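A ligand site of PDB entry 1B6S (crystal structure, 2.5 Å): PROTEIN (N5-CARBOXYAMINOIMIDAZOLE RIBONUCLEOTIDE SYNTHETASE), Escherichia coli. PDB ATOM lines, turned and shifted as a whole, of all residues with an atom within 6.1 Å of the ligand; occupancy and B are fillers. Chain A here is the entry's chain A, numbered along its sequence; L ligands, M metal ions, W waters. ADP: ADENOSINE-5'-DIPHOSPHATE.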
ATOM      1  N   ARG A  80       9.162   4.415 -19.703  1.00  0.00           N
ATOM      2  CA  ARG A  80       8.519   3.105 -19.675  1.00  0.00           C
ATOM      3  C   ARG A  80       7.035   3.189 -19.233  1.00  0.00           C
ATOM      4  O   ARG A  80       6.158   2.403 -19.644  1.00  0.00           O
ATOM      5  CB  ARG A  80       9.304   2.156 -18.772  1.00  0.00           C
ATOM      6  CG  ARG A  80       9.987   1.015 -19.515  1.00  0.00           C
ATOM      7  CD  ARG A  80      10.784   0.117 -18.564  1.00  0.00           C
ATOM      8  NE  ARG A  80      12.166  -0.103 -18.988  1.00  0.00           N
ATOM      9  CZ  ARG A  80      12.525  -0.855 -20.021  1.00  0.00           C
ATOM     10  NH1 ARG A  80      11.620  -1.512 -20.783  1.00  0.00           N
ATOM     11  NH2 ARG A  80      13.827  -0.968 -20.279  1.00  0.00           N
ATOM     12  N   ALA A  95       2.499  -7.148 -21.096  1.00  0.00           N
ATOM     13  CA  ALA A  95       2.433  -7.703 -19.741  1.00  0.00           C
ATOM     14  C   ALA A  95       1.817  -6.750 -18.735  1.00  0.00           C
ATOM     15  O   ALA A  95       2.172  -5.561 -18.661  1.00  0.00           O
ATOM     16  CB  ALA A  95       3.765  -8.203 -19.180  1.00  0.00           C
ATOM     17  N   ILE A 118       8.625  -8.527 -12.100  1.00  0.00           N
ATOM     18  CA  ILE A 118       9.729  -7.893 -12.795  1.00  0.00           C
ATOM     19  C   ILE A 118       9.594  -6.372 -12.738  1.00  0.00           C
ATOM     20  O   ILE A 118       8.581  -5.813 -13.142  1.00  0.00           O
ATOM     21  CB  ILE A 118       9.858  -8.404 -14.205  1.00  0.00           C
ATOM     22  CG1 ILE A 118      10.667  -9.691 -14.178  1.00  0.00           C
ATOM     23  CG2 ILE A 118      10.626  -7.369 -15.005  1.00  0.00           C
ATOM     24  CD1 ILE A 118       9.851 -10.912 -14.597  1.00  0.00           C
ATOM     25  N   LYS A 120      11.410  -2.515 -13.432  1.00  0.00           N
ATOM     26  CA  LYS A 120      12.358  -1.764 -14.231  1.00  0.00           C
ATOM     27  C   LYS A 120      12.197  -0.281 -14.048  1.00  0.00           C
ATOM     28  O   LYS A 120      11.119   0.216 -13.659  1.00  0.00           O
ATOM     29  CB  LYS A 120      12.269  -2.000 -15.737  1.00  0.00           C
ATOM     30  CG  LYS A 120      12.139  -3.438 -16.204  1.00  0.00           C
ATOM     31  CD  LYS A 120      11.781  -3.546 -17.674  1.00  0.00           C
ATOM     32  CE  LYS A 120      10.896  -4.737 -18.020  1.00  0.00           C
ATOM     33  NZ  LYS A 120      11.157  -5.295 -19.363  1.00  0.00           N
ATOM     34  N   GLY A 125      17.202   3.041 -18.261  1.00  0.00           N
ATOM     35  CA  GLY A 125      17.322   1.595 -18.082  1.00  0.00           C
ATOM     36  C   GLY A 125      17.705   1.321 -16.635  1.00  0.00           C
ATOM     37  O   GLY A 125      18.658   0.596 -16.362  1.00  0.00           O
ATOM     38  N   GLY A 130      18.653  -2.466 -14.761  1.00  0.00           N
ATOM     39  CA  GLY A 130      17.360  -1.819 -14.670  1.00  0.00           C
ATOM     40  C   GLY A 130      16.187  -2.794 -14.602  1.00  0.00           C
ATOM     41  O   GLY A 130      15.058  -2.499 -15.035  1.00  0.00           O
ATOM     42  N   GLN A 131      16.474  -3.968 -14.047  1.00  0.00           N
ATOM     43  CA  GLN A 131      15.478  -4.987 -13.888  1.00  0.00           C
ATOM     44  C   GLN A 131      15.796  -5.922 -12.730  1.00  0.00           C
ATOM     45  O   GLN A 131      16.840  -6.575 -12.686  1.00  0.00           O
ATOM     46  CB  GLN A 131      15.157  -5.745 -15.188  1.00  0.00           C
ATOM     47  CG  GLN A 131      14.493  -7.109 -14.922  1.00  0.00           C
ATOM     48  CD  GLN A 131      14.435  -7.926 -16.187  1.00  0.00           C
ATOM     49  OE1 GLN A 131      14.227  -9.140 -16.134  1.00  0.00           O
ATOM     50  NE2 GLN A 131      14.608  -7.230 -17.317  1.00  0.00           N
ATOM     51  N   ARG A 133      14.034  -9.029 -10.456  1.00  0.00           N
ATOM     52  CA  ARG A 133      13.027 -10.105 -10.386  1.00  0.00           C
ATOM     53  C   ARG A 133      12.770 -10.511  -8.948  1.00  0.00           C
ATOM     54  O   ARG A 133      13.442 -11.380  -8.412  1.00  0.00           O
ATOM     55  CB  ARG A 133      13.394 -11.376 -11.144  1.00  0.00           C
ATOM     56  CG  ARG A 133      13.530 -11.127 -12.641  1.00  0.00           C
ATOM     57  CD  ARG A 133      14.437 -12.110 -13.354  1.00  0.00           C
ATOM     58  NE  ARG A 133      14.326 -12.015 -14.807  1.00  0.00           N
ATOM     59  CZ  ARG A 133      14.173 -13.077 -15.607  1.00  0.00           C
ATOM     60  NH1 ARG A 133      14.118 -14.297 -15.094  1.00  0.00           N
ATOM     61  NH2 ARG A 133      14.070 -12.904 -16.940  1.00  0.00           N
ATOM     62  N   GLU A 153       5.770  -5.310 -13.678  1.00  0.00           N
ATOM     63  CA  GLU A 153       5.120  -6.259 -14.595  1.00  0.00           C
ATOM     64  C   GLU A 153       5.065  -7.706 -14.182  1.00  0.00           C
ATOM     65  O   GLU A 153       5.949  -8.262 -13.532  1.00  0.00           O
ATOM     66  CB  GLU A 153       5.858  -6.335 -15.922  1.00  0.00           C
ATOM     67  CG  GLU A 153       5.655  -5.096 -16.786  1.00  0.00           C
ATOM     68  CD  GLU A 153       6.459  -5.153 -18.053  1.00  0.00           C
ATOM     69  OE1 GLU A 153       6.999  -6.331 -18.274  1.00  0.00           O
ATOM     70  OE2 GLU A 153       6.609  -4.179 -18.785  1.00  0.00           O
ATOM     71  N   GLN A 154       4.060  -8.351 -14.733  1.00  0.00           N
ATOM     72  CA  GLN A 154       3.838  -9.738 -14.505  1.00  0.00           C
ATOM     73  C   GLN A 154       4.910 -10.539 -15.186  1.00  0.00           C
ATOM     74  O   GLN A 154       5.219 -10.280 -16.348  1.00  0.00           O
ATOM     75  CB  GLN A 154       2.476 -10.162 -15.066  1.00  0.00           C
ATOM     76  CG  GLN A 154       2.398 -11.677 -15.227  1.00  0.00           C
ATOM     77  CD  GLN A 154       1.022 -12.088 -15.695  1.00  0.00           C
ATOM     78  OE1 GLN A 154       0.030 -11.456 -15.331  1.00  0.00           O
ATOM     79  NE2 GLN A 154       0.968 -13.142 -16.502  1.00  0.00           N
ATOM     80  N   GLY A 155       5.474 -11.496 -14.437  1.00  0.00           N
ATOM     81  CA  GLY A 155       6.500 -12.379 -14.967  1.00  0.00           C
ATOM     82  C   GLY A 155       5.877 -13.197 -16.082  1.00  0.00           C
ATOM     83  O   GLY A 155       4.921 -13.965 -15.871  1.00  0.00           O
ATOM     84  N   ILE A 156       6.430 -12.976 -17.267  1.00  0.00           N
ATOM     85  CA  ILE A 156       5.930 -13.571 -18.486  1.00  0.00           C
ATOM     86  C   ILE A 156       6.774 -14.745 -18.902  1.00  0.00           C
ATOM     87  O   ILE A 156       7.990 -14.653 -19.074  1.00  0.00           O
ATOM     88  CB  ILE A 156       5.815 -12.570 -19.648  1.00  0.00           C
ATOM     89  CG1 ILE A 156       4.905 -11.350 -19.384  1.00  0.00           C
ATOM     90  CG2 ILE A 156       5.395 -13.294 -20.921  1.00  0.00           C
ATOM     91  CD1 ILE A 156       3.510 -11.650 -18.803  1.00  0.00           C
ATOM     92  N   ASN A 157       6.086 -15.852 -19.080  1.00  0.00           N
ATOM     93  CA  ASN A 157       6.719 -17.071 -19.489  1.00  0.00           C
ATOM     94  C   ASN A 157       6.495 -17.203 -20.982  1.00  0.00           C
ATOM     95  O   ASN A 157       5.446 -17.654 -21.456  1.00  0.00           O
ATOM     96  CB  ASN A 157       6.162 -18.303 -18.725  1.00  0.00           C
ATOM     97  CG  ASN A 157       6.032 -18.069 -17.232  1.00  0.00           C
ATOM     98  OD1 ASN A 157       7.025 -17.759 -16.524  1.00  0.00           O
ATOM     99  ND2 ASN A 157       4.796 -18.243 -16.760  1.00  0.00           N
ATOM    100  N   PHE A 158       7.489 -16.747 -21.727  1.00  0.00           N
ATOM    101  CA  PHE A 158       7.417 -16.748 -23.166  1.00  0.00           C
ATOM    102  C   PHE A 158       8.164 -17.936 -23.687  1.00  0.00           C
ATOM    103  O   PHE A 158       9.038 -18.458 -23.035  1.00  0.00           O
ATOM    104  CB  PHE A 158       8.005 -15.452 -23.763  1.00  0.00           C
ATOM    105  CG  PHE A 158       9.432 -15.143 -23.335  1.00  0.00           C
ATOM    106  CD1 PHE A 158      10.501 -15.660 -24.067  1.00  0.00           C
ATOM    107  CD2 PHE A 158       9.708 -14.337 -22.230  1.00  0.00           C
ATOM    108  CE1 PHE A 158      11.825 -15.393 -23.712  1.00  0.00           C
ATOM    109  CE2 PHE A 158      11.018 -14.043 -21.862  1.00  0.00           C
ATOM    110  CZ  PHE A 158      12.073 -14.575 -22.602  1.00  0.00           C
ATOM    111  N   GLU A 161      11.746 -14.990 -27.964  1.00  0.00           N
ATOM    112  CA  GLU A 161      11.768 -13.527 -28.026  1.00  0.00           C
ATOM    113  C   GLU A 161      11.959 -13.104 -29.463  1.00  0.00           C
ATOM    114  O   GLU A 161      12.771 -13.676 -30.171  1.00  0.00           O
ATOM    115  CB  GLU A 161      12.846 -12.865 -27.132  1.00  0.00           C
ATOM    116  CG  GLU A 161      12.609 -13.065 -25.617  1.00  0.00           C
ATOM    117  CD  GLU A 161      13.511 -12.210 -24.785  1.00  0.00           C
ATOM    118  OE1 GLU A 161      13.019 -11.007 -24.563  1.00  0.00           O
ATOM    119  OE2 GLU A 161      14.592 -12.600 -24.373  1.00  0.00           O
ATOM    120  N   HIS A 184      18.879 -13.237 -25.243  1.00  0.00           N
ATOM    121  CA  HIS A 184      19.418 -12.432 -24.163  1.00  0.00           C
ATOM    122  C   HIS A 184      20.027 -13.253 -23.058  1.00  0.00           C
ATOM    123  O   HIS A 184      19.513 -14.302 -22.668  1.00  0.00           O
ATOM    124  CB  HIS A 184      18.308 -11.613 -23.486  1.00  0.00           C
ATOM    125  CG  HIS A 184      17.756 -10.598 -24.389  1.00  0.00           C
ATOM    126  ND1 HIS A 184      16.719 -10.881 -25.252  1.00  0.00           N
ATOM    127  CD2 HIS A 184      18.144  -9.319 -24.576  1.00  0.00           C
ATOM    128  CE1 HIS A 184      16.498  -9.786 -25.950  1.00  0.00           C
ATOM    129  NE2 HIS A 184      17.323  -8.827 -25.551  1.00  0.00           N
ATOM    130  N   GLY A 187      20.548 -10.317 -19.184  1.00  0.00           N
ATOM    131  CA  GLY A 187      19.834  -9.139 -19.665  1.00  0.00           C
ATOM    132  C   GLY A 187      20.461  -8.381 -20.814  1.00  0.00           C
ATOM    133  O   GLY A 187      20.143  -7.212 -21.048  1.00  0.00           O
ATOM    134  N   GLU A 226      10.316  -4.887 -29.512  1.00  0.00           N
ATOM    135  CA  GLU A 226      10.653  -6.158 -28.884  1.00  0.00           C
ATOM    136  C   GLU A 226       9.406  -6.815 -28.358  1.00  0.00           C
ATOM    137  O   GLU A 226       8.600  -6.229 -27.611  1.00  0.00           O
ATOM    138  CB  GLU A 226      11.776  -6.068 -27.782  1.00  0.00           C
ATOM    139  CG  GLU A 226      13.092  -5.455 -28.300  1.00  0.00           C
ATOM    140  CD  GLU A 226      14.317  -5.774 -27.487  1.00  0.00           C
ATOM    141  OE1 GLU A 226      14.469  -4.955 -26.472  1.00  0.00           O
ATOM    142  OE2 GLU A 226      15.099  -6.678 -27.772  1.00  0.00           O
ATOM    143  N   PHE A 228       7.491 -10.741 -27.109  1.00  0.00           N
ATOM    144  CA  PHE A 228       7.574 -12.037 -26.497  1.00  0.00           C
ATOM    145  C   PHE A 228       6.624 -12.939 -27.220  1.00  0.00           C
ATOM    146  O   PHE A 228       5.517 -12.558 -27.576  1.00  0.00           O
ATOM    147  CB  PHE A 228       7.150 -12.095 -25.002  1.00  0.00           C
ATOM    148  CG  PHE A 228       8.019 -11.336 -24.031  1.00  0.00           C
ATOM    149  CD1 PHE A 228       9.408 -11.494 -24.019  1.00  0.00           C
ATOM    150  CD2 PHE A 228       7.445 -10.471 -23.112  1.00  0.00           C
ATOM    151  CE1 PHE A 228      10.195 -10.783 -23.125  1.00  0.00           C
ATOM    152  CE2 PHE A 228       8.221  -9.761 -22.196  1.00  0.00           C
ATOM    153  CZ  PHE A 228       9.605  -9.920 -22.214  1.00  0.00           C
ATOM    154  N   ASN A 237       7.022  -5.980 -25.660  1.00  0.00           N
ATOM    155  CA  ASN A 237       7.794  -5.754 -24.487  1.00  0.00           C
ATOM    156  C   ASN A 237       8.311  -4.326 -24.453  1.00  0.00           C
ATOM    157  O   ASN A 237       8.018  -3.582 -23.543  1.00  0.00           O
ATOM    158  CB  ASN A 237       8.959  -6.767 -24.320  1.00  0.00           C
ATOM    159  CG  ASN A 237      10.016  -6.292 -23.300  1.00  0.00           C
ATOM    160  OD1 ASN A 237       9.727  -5.834 -22.165  1.00  0.00           O
ATOM    161  ND2 ASN A 237      11.269  -6.408 -23.681  1.00  0.00           N
ATOM    162  N   GLU A 238       9.091  -3.983 -25.475  1.00  0.00           N
ATOM    163  CA  GLU A 238       9.753  -2.699 -25.496  1.00  0.00           C
ATOM    164  C   GLU A 238       9.826  -2.080 -26.903  1.00  0.00           C
ATOM    165  O   GLU A 238       9.815  -2.768 -27.922  1.00  0.00           O
ATOM    166  CB  GLU A 238      11.180  -3.001 -25.003  1.00  0.00           C
ATOM    167  CG  GLU A 238      11.829  -2.017 -24.035  1.00  0.00           C
ATOM    168  CD  GLU A 238      13.310  -2.311 -23.887  1.00  0.00           C
ATOM    169  OE1 GLU A 238      13.643  -3.524 -24.284  1.00  0.00           O
ATOM    170  OE2 GLU A 238      14.112  -1.489 -23.474  1.00  0.00           O
HETATM  171  PB  ADP L   1      16.528  -3.853 -21.773  1.00  0.00           P
HETATM  172  O1B ADP L   1      17.226  -4.350 -20.552  1.00  0.00           O
HETATM  173  O2B ADP L   1      16.244  -2.393 -21.649  1.00  0.00           O
HETATM  174  O3B ADP L   1      17.254  -4.179 -23.066  1.00  0.00           O
HETATM  175  PA  ADP L   1      13.947  -5.143 -21.121  1.00  0.00           P
HETATM  176  O1A ADP L   1      13.820  -4.262 -19.946  1.00  0.00           O
HETATM  177  O2A ADP L   1      12.604  -5.175 -21.769  1.00  0.00           O
HETATM  178  O3A ADP L   1      15.125  -4.700 -22.051  1.00  0.00           O
HETATM  179  O5' ADP L   1      14.295  -6.611 -20.596  1.00  0.00           O
HETATM  180  C5' ADP L   1      15.385  -7.383 -21.158  1.00  0.00           C
HETATM  181  C4' ADP L   1      15.032  -8.850 -20.977  1.00  0.00           C
HETATM  182  O4' ADP L   1      14.316  -9.055 -19.734  1.00  0.00           O
HETATM  183  C3' ADP L   1      13.990  -9.367 -21.929  1.00  0.00           C
HETATM  184  O3' ADP L   1      14.348  -9.152 -23.364  1.00  0.00           O
HETATM  185  C2' ADP L   1      13.776 -10.700 -21.225  1.00  0.00           C
HETATM  186  O2' ADP L   1      14.921 -11.658 -21.146  1.00  0.00           O
HETATM  187  C1' ADP L   1      13.492 -10.180 -19.828  1.00  0.00           C
HETATM  188  N9  ADP L   1      12.124  -9.703 -19.540  1.00  0.00           N
HETATM  189  C8  ADP L   1      11.701  -8.387 -19.493  1.00  0.00           C
HETATM  190  N7  ADP L   1      10.459  -8.250 -19.002  1.00  0.00           N
HETATM  191  C5  ADP L   1      10.054  -9.559 -18.762  1.00  0.00           C
HETATM  192  C6  ADP L   1       8.829 -10.044 -18.281  1.00  0.00           C
HETATM  193  N6  ADP L   1       7.825  -9.236 -17.947  1.00  0.00           N
HETATM  194  N1  ADP L   1       8.726 -11.407 -18.185  1.00  0.00           N
HETATM  195  C2  ADP L   1       9.808 -12.181 -18.553  1.00  0.00           C
HETATM  196  N3  ADP L   1      10.973 -11.814 -19.013  1.00  0.00           N
HETATM  197  C4  ADP L   1      11.047 -10.467 -19.114  1.00  0.00           C
HETATM  198 MG    MG M   1      15.318  -6.718 -24.247  1.00  0.00          MG
HETATM  199  O   HOH W   1      18.081 -12.324 -20.001  1.00  0.00           O
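Water W1 bridges the backbone NH of Gly 187 and an oxygen (O2') of the ligand.
The side-chain carboxylate of Glu 161 is in hydrogen-bond range of a ring nitrogen (ND1) of His 184 (2.9 Å).
OD1 of Asn 237 is in hydrogen-bond range of NZ of Lys 120 (3.2 Å).
The backbone carbonyl oxygen (O) of Glu 226 is in hydrogen-bond range of the backbone NH (N) of Asn 237, 2.5 Å away.
The guanidinium group (NH2) of Arg 80 is in salt-bridge range of the side-chain carboxylate (OE2) of Glu 238 (3.2 Å).
The backbone NH of Glu 226 sits at hydrogen-bond distance from the backbone carbonyl oxygen of Glu 238.
The backbone NH (N) of Glu 153 sits at hydrogen-bond distance from the backbone carbonyl oxygen (O) of Ile 118, at 2.9 Å.
The guanidinium group (NE) of Arg 133 lies within hydrogen-bond range of the side-chain amide oxygen (OE1) of Gln 131.
Ile 118 touches the ligand.
NH2 of Arg 133 touches N3 of the ligand (3.9 Å).
C of Gly 155 touches N1 of the ligand (3.97 Å).
CE2 of Phe 158 touches N3 of the ligand, at 3.6 Å.
Phe 228 touches the ligand (CZ to C4, 3.5 Å).
Hydrophobic or aromatic side chains that line the ligand: Ile 118, Ile 156, Phe 158, His 184 and Phe 228.
The nearest printed residue that does not touch the ligand is Gly 187 (4.1 Å).
An oxygen (O3') of the ligand is in hydrogen-bond range of the side-chain carboxylate (OE1) of Glu 161, 2.6 Å away.
The side-chain amide nitrogen (ND2) of Asn 237 lies within hydrogen-bond range of an oxygen (O2A) of the ligand.
The side-chain amino group (NZ) of Lys 120 is in salt-bridge range of an oxygen (O2A) of the ligand, at 2.8 Å.
The side-chain carboxylate (OE2) of Glu 238 sits close to an oxygen (O2B) of the ligand (2.9 Å).
The backbone NH of Ile 156 is in hydrogen-bond range of a nitrogen (N1) of the ligand, at 2.9 Å.
A nitrogen (N6) of the ligand lies within hydrogen-bond range of the side-chain carboxylate (OE1) of Glu 153.
The side-chain amide nitrogen of Gln 131 sits at hydrogen-bond distance from an oxygen (O4') of the ligand (3.0 Å).
O2B of the ligand is in salt-bridge range of NH2 of Arg 80 (3.1 Å).
O of Gln 154 sits at hydrogen-bond distance from N6 of the ligand (3.2 Å).
A ring nitrogen (ND1) of His 184 lies close to an oxygen (O3') of the ligand (3.5 Å).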
